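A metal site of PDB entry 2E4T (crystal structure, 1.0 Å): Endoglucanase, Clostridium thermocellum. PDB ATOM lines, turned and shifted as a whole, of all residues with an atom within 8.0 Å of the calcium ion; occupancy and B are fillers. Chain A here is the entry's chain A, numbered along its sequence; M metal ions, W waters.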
ATOM      1  N   ASN A  52      25.177   3.589  24.573  1.00  0.00           N
ATOM      2  CA  ASN A  52      24.834   3.061  23.253  1.00  0.00           C
ATOM      3  C   ASN A  52      25.792   3.659  22.234  1.00  0.00           C
ATOM      4  O   ASN A  52      25.698   4.844  21.910  1.00  0.00           O
ATOM      5  CB  ASN A  52      23.388   3.444  22.933  1.00  0.00           C
ATOM      6  CG  ASN A  52      22.910   2.904  21.614  1.00  0.00           C
ATOM      7  OD1 ASN A  52      23.708   2.539  20.743  1.00  0.00           O
ATOM      8  ND2 ASN A  52      21.583   2.839  21.472  1.00  0.00           N
ATOM      9  N   TRP A  53      26.702   2.841  21.680  1.00  0.00           N
ATOM     10  CA  TRP A  53      27.697   3.398  20.779  1.00  0.00           C
ATOM     11  C   TRP A  53      27.065   3.959  19.486  1.00  0.00           C
ATOM     12  O   TRP A  53      27.692   4.760  18.779  1.00  0.00           O
ATOM     13  CB  TRP A  53      28.750   2.331  20.410  1.00  0.00           C
ATOM     14  CG  TRP A  53      28.301   1.311  19.406  1.00  0.00           C
ATOM     15  CD1 TRP A  53      27.521   0.210  19.629  1.00  0.00           C
ATOM     16  CD2 TRP A  53      28.658   1.286  18.009  1.00  0.00           C
ATOM     17  NE1 TRP A  53      27.354  -0.508  18.444  1.00  0.00           N
ATOM     18  CE2 TRP A  53      28.034   0.135  17.456  1.00  0.00           C
ATOM     19  CE3 TRP A  53      29.447   2.091  17.190  1.00  0.00           C
ATOM     20  CZ2 TRP A  53      28.228  -0.232  16.116  1.00  0.00           C
ATOM     21  CZ3 TRP A  53      29.631   1.738  15.867  1.00  0.00           C
ATOM     22  CH2 TRP A  53      29.029   0.579  15.349  1.00  0.00           C
ATOM     23  N   GLU A  54      25.848   3.492  19.145  1.00  0.00           N
ATOM     24  CA  GLU A  54      25.272   3.934  17.880  1.00  0.00           C
ATOM     25  C   GLU A  54      24.873   5.401  17.891  1.00  0.00           C
ATOM     26  O   GLU A  54      24.917   6.057  16.864  1.00  0.00           O
ATOM     27  CB  GLU A  54      24.045   3.088  17.519  1.00  0.00           C
ATOM     28  CG  GLU A  54      24.343   1.604  17.420  1.00  0.00           C
ATOM     29  CD  GLU A  54      23.130   0.786  16.939  1.00  0.00           C
ATOM     30  OE1 GLU A  54      21.972   1.330  16.980  1.00  0.00           O
ATOM     31  OE2 GLU A  54      23.312  -0.380  16.528  1.00  0.00           O
ATOM     32  N   ASN A  55      24.437   5.888  19.078  1.00  0.00           N
ATOM     33  CA  ASN A  55      23.904   7.270  19.194  1.00  0.00           C
ATOM     34  C   ASN A  55      24.479   8.041  20.358  1.00  0.00           C
ATOM     35  O   ASN A  55      24.141   9.220  20.519  1.00  0.00           O
ATOM     36  CB  ASN A  55      22.383   7.234  19.217  1.00  0.00           C
ATOM     37  CG  ASN A  55      21.883   6.415  20.353  1.00  0.00           C
ATOM     38  OD1 ASN A  55      22.540   6.245  21.386  1.00  0.00           O
ATOM     39  ND2 ASN A  55      20.672   5.874  20.181  1.00  0.00           N
ATOM     40  N   LYS A 135      17.546  -0.386  23.836  1.00  0.00           N
ATOM     41  CA  LYS A 135      17.888  -1.328  22.785  1.00  0.00           C
ATOM     42  C   LYS A 135      18.571  -2.535  23.421  1.00  0.00           C
ATOM     43  O   LYS A 135      19.393  -2.384  24.358  1.00  0.00           O
ATOM     44  CB  LYS A 135      18.851  -0.691  21.781  1.00  0.00           C
ATOM     45  CG  LYS A 135      18.311   0.535  21.086  1.00  0.00           C
ATOM     46  CD  LYS A 135      17.059   0.283  20.285  1.00  0.00           C
ATOM     47  CE  LYS A 135      16.571   1.550  19.568  1.00  0.00           C
ATOM     48  NZ  LYS A 135      15.308   1.251  18.797  1.00  0.00           N
ATOM     49  N   GLU A 136      18.225  -3.735  22.955  1.00  0.00           N
ATOM     50  CA  GLU A 136      18.830  -4.945  23.446  1.00  0.00           C
ATOM     51  C   GLU A 136      20.252  -5.116  22.884  1.00  0.00           C
ATOM     52  O   GLU A 136      20.436  -4.974  21.672  1.00  0.00           O
ATOM     53  CB  GLU A 136      17.954  -6.152  23.022  1.00  0.00           C
ATOM     54  CG  GLU A 136      18.489  -7.489  23.563  1.00  0.00           C
ATOM     55  CD  GLU A 136      17.772  -8.690  23.041  1.00  0.00           C
ATOM     56  OE1 GLU A 136      16.518  -8.642  22.896  1.00  0.00           O
ATOM     57  OE2 GLU A 136      18.455  -9.726  22.756  1.00  0.00           O
ATOM     58  N   LYS A 141      26.746  -9.818  15.962  1.00  0.00           N
ATOM     59  CA  LYS A 141      25.731  -9.441  14.971  1.00  0.00           C
ATOM     60  C   LYS A 141      25.267 -10.624  14.123  1.00  0.00           C
ATOM     61  O   LYS A 141      24.076 -10.728  13.799  1.00  0.00           O
ATOM     62  CB  LYS A 141      26.268  -8.329  14.096  1.00  0.00           C
ATOM     63  CG  LYS A 141      25.225  -7.735  13.158  1.00  0.00           C
ATOM     64  CD  LYS A 141      25.753  -6.591  12.379  1.00  0.00           C
ATOM     65  CE  LYS A 141      24.672  -5.873  11.562  1.00  0.00           C
ATOM     66  NZ  LYS A 141      25.209  -4.837  10.667  1.00  0.00           N
ATOM     67  N   THR A 148      28.048   2.305   9.622  1.00  0.00           N
ATOM     68  CA  THR A 148      26.895   3.172   9.883  1.00  0.00           C
ATOM     69  C   THR A 148      25.826   2.264  10.463  1.00  0.00           C
ATOM     70  O   THR A 148      24.949   1.752   9.743  1.00  0.00           O
ATOM     71  CB  THR A 148      26.373   3.870   8.625  1.00  0.00           C
ATOM     72  OG1 THR A 148      26.169   2.935   7.574  1.00  0.00           O
ATOM     73  CG2 THR A 148      27.377   4.812   8.093  1.00  0.00           C
ATOM     74  N   PRO A 149      25.933   1.953  11.774  1.00  0.00           N
ATOM     75  CA  PRO A 149      24.991   0.996  12.349  1.00  0.00           C
ATOM     76  C   PRO A 149      23.580   1.523  12.262  1.00  0.00           C
ATOM     77  O   PRO A 149      23.333   2.717  12.209  1.00  0.00           O
ATOM     78  CB  PRO A 149      25.457   0.915  13.815  1.00  0.00           C
ATOM     79  CG  PRO A 149      26.151   2.210  14.102  1.00  0.00           C
ATOM     80  CD  PRO A 149      26.898   2.454  12.783  1.00  0.00           C
ATOM     81  N   ASP A 150      22.644   0.593  12.203  1.00  0.00           N
ATOM     82  CA  ASP A 150      21.224   0.938  12.049  1.00  0.00           C
ATOM     83  C   ASP A 150      20.630   1.389  13.355  1.00  0.00           C
ATOM     84  O   ASP A 150      20.484   0.591  14.269  1.00  0.00           O
ATOM     85  CB  ASP A 150      20.475  -0.272  11.501  1.00  0.00           C
ATOM     86  CG  ASP A 150      19.032  -0.002  11.204  1.00  0.00           C
ATOM     87  OD1 ASP A 150      18.517   1.125  11.478  1.00  0.00           O
ATOM     88  OD2 ASP A 150      18.399  -0.893  10.597  1.00  0.00           O
ATOM     89  N   THR A 151      20.324   2.667  13.465  1.00  0.00           N
ATOM     90  CA  THR A 151      19.791   3.204  14.676  1.00  0.00           C
ATOM     91  C   THR A 151      18.281   2.936  14.800  1.00  0.00           C
ATOM     92  O   THR A 151      17.699   3.215  15.858  1.00  0.00           O
ATOM     93  CB  THR A 151      20.032   4.714  14.819  1.00  0.00           C
ATOM     94  OG1 THR A 151      19.532   5.332  13.618  1.00  0.00           O
ATOM     95  CG2 THR A 151      21.509   4.997  14.964  1.00  0.00           C
ATOM     96  N   GLU A 152      17.652   2.358  13.778  1.00  0.00           N
ATOM     97  CA  GLU A 152      16.196   2.209  13.770  1.00  0.00           C
ATOM     98  C   GLU A 152      15.715   0.829  14.269  1.00  0.00           C
ATOM     99  O   GLU A 152      14.508   0.620  14.550  1.00  0.00           O
ATOM    100  CB  GLU A 152      15.656   2.584  12.377  1.00  0.00           C
ATOM    101  CG  GLU A 152      16.076   4.034  11.978  1.00  0.00           C
ATOM    102  CD  GLU A 152      15.820   5.075  13.119  1.00  0.00           C
ATOM    103  OE1 GLU A 152      14.654   5.212  13.578  1.00  0.00           O
ATOM    104  OE2 GLU A 152      16.780   5.741  13.587  1.00  0.00           O
ATOM    105  N   ASP A 153      16.625  -0.132  14.359  1.00  0.00           N
ATOM    106  CA  ASP A 153      16.268  -1.446  14.749  1.00  0.00           C
ATOM    107  C   ASP A 153      16.331  -1.555  16.268  1.00  0.00           C
ATOM    108  O   ASP A 153      16.551  -0.567  16.990  1.00  0.00           O
ATOM    109  CB  ASP A 153      17.091  -2.489  13.999  1.00  0.00           C
ATOM    110  CG  ASP A 153      18.548  -2.512  14.380  1.00  0.00           C
ATOM    111  OD1 ASP A 153      18.904  -1.819  15.346  1.00  0.00           O
ATOM    112  OD2 ASP A 153      19.340  -3.214  13.679  1.00  0.00           O
ATOM    113  N   ASP A 154      16.100  -2.760  16.753  1.00  0.00           N
ATOM    114  CA  ASP A 154      15.914  -3.006  18.191  1.00  0.00           C
ATOM    115  C   ASP A 154      17.192  -3.411  18.941  1.00  0.00           C
ATOM    116  O   ASP A 154      17.139  -3.634  20.156  1.00  0.00           O
ATOM    117  CB  ASP A 154      14.852  -4.102  18.430  1.00  0.00           C
ATOM    118  CG  ASP A 154      13.473  -3.700  17.949  1.00  0.00           C
ATOM    119  OD1 ASP A 154      13.246  -2.480  17.792  1.00  0.00           O
ATOM    120  OD2 ASP A 154      12.633  -4.614  17.786  1.00  0.00           O
ATOM    121  N   TYR A 155      18.339  -3.449  18.239  1.00  0.00           N
ATOM    122  CA  TYR A 155      19.520  -4.118  18.748  1.00  0.00           C
ATOM    123  C   TYR A 155      20.746  -3.261  18.593  1.00  0.00           C
ATOM    124  O   TYR A 155      20.851  -2.482  17.669  1.00  0.00           O
ATOM    125  CB  TYR A 155      19.803  -5.436  17.983  1.00  0.00           C
ATOM    126  CG  TYR A 155      18.614  -6.366  18.114  1.00  0.00           C
ATOM    127  CD1 TYR A 155      18.392  -7.026  19.309  1.00  0.00           C
ATOM    128  CD2 TYR A 155      17.703  -6.541  17.078  1.00  0.00           C
ATOM    129  CE1 TYR A 155      17.254  -7.755  19.518  1.00  0.00           C
ATOM    130  CE2 TYR A 155      16.556  -7.342  17.264  1.00  0.00           C
ATOM    131  CZ  TYR A 155      16.349  -7.919  18.481  1.00  0.00           C
ATOM    132  OH  TYR A 155      15.214  -8.668  18.599  1.00  0.00           O
ATOM    133  N   VAL A 156      21.704  -3.474  19.519  1.00  0.00           N
ATOM    134  CA  VAL A 156      23.039  -2.860  19.426  1.00  0.00           C
ATOM    135  C   VAL A 156      24.048  -4.001  19.570  1.00  0.00           C
ATOM    136  O   VAL A 156      23.901  -4.834  20.462  1.00  0.00           O
ATOM    137  CB  VAL A 156      23.200  -1.805  20.526  1.00  0.00           C
ATOM    138  CG1 VAL A 156      24.569  -1.251  20.576  1.00  0.00           C
ATOM    139  CG2 VAL A 156      22.174  -0.630  20.300  1.00  0.00           C
ATOM    140  N   TYR A 157      25.050  -4.034  18.688  1.00  0.00           N
ATOM    141  CA  TYR A 157      25.932  -5.185  18.600  1.00  0.00           C
ATOM    142  C   TYR A 157      27.352  -4.825  19.093  1.00  0.00           C
ATOM    143  O   TYR A 157      27.967  -3.883  18.574  1.00  0.00           O
ATOM    144  CB  TYR A 157      26.016  -5.682  17.149  1.00  0.00           C
ATOM    145  CG  TYR A 157      24.655  -6.109  16.651  1.00  0.00           C
ATOM    146  CD1 TYR A 157      24.114  -7.311  17.038  1.00  0.00           C
ATOM    147  CD2 TYR A 157      23.904  -5.304  15.786  1.00  0.00           C
ATOM    148  CE1 TYR A 157      22.864  -7.722  16.591  1.00  0.00           C
ATOM    149  CE2 TYR A 157      22.636  -5.695  15.354  1.00  0.00           C
ATOM    150  CZ  TYR A 157      22.139  -6.937  15.757  1.00  0.00           C
ATOM    151  OH  TYR A 157      20.892  -7.361  15.358  1.00  0.00           O
ATOM    152  N   GLU A 160      30.163  -5.305  16.418  1.00  0.00           N
ATOM    153  CA  GLU A 160      30.112  -4.256  15.434  1.00  0.00           C
ATOM    154  C   GLU A 160      30.766  -2.969  15.971  1.00  0.00           C
ATOM    155  O   GLU A 160      31.470  -2.254  15.243  1.00  0.00           O
ATOM    156  CB  GLU A 160      28.684  -4.021  14.978  1.00  0.00           C
ATOM    157  CG  GLU A 160      28.601  -3.109  13.767  1.00  0.00           C
ATOM    158  CD  GLU A 160      27.185  -3.063  13.199  1.00  0.00           C
ATOM    159  OE1 GLU A 160      26.223  -2.771  13.976  1.00  0.00           O
ATOM    160  OE2 GLU A 160      27.028  -3.326  11.974  1.00  0.00           O
HETATM  161 CA    CA M   1      20.939  -0.793  16.080  1.00  0.00          CA
HETATM  162  O   HOH W   1      19.212   0.254  17.354  1.00  0.00           O
HETATM  163  O   HOH W   2      21.810  -2.409  14.569  1.00  0.00           O
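Of the 18 residues printed, 4 come within 4 Å of the calcium ion.
The nearest printed residue that does not touch the calcium ion is Thr 151 (4.4 Å).
The calcium ion is bound by O of Tyr 155 (2.3 Å), O of Asp 150 (2.3 Å), water W2 (2.4 Å), water W1 (2.4 Å), OD1 of Asp 153 (2.4 Å), OE2 of Glu 54 (2.4 Å) and OE1 of Glu 54 (2.5 Å).
The side-chain carboxylate of Asp 150 lies within hydrogen-bond range of the backbone NH of Glu 152 (2.7 Å).
The backbone NH (N) of Glu 54 is in hydrogen-bond range of the side-chain amide oxygen (OD1) of Asn 52 (2.8 Å).
The side-chain amino group (NZ) of Lys 135 sits at hydrogen-bond distance from the backbone carbonyl oxygen (O) of Asp 153 (2.8 Å).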
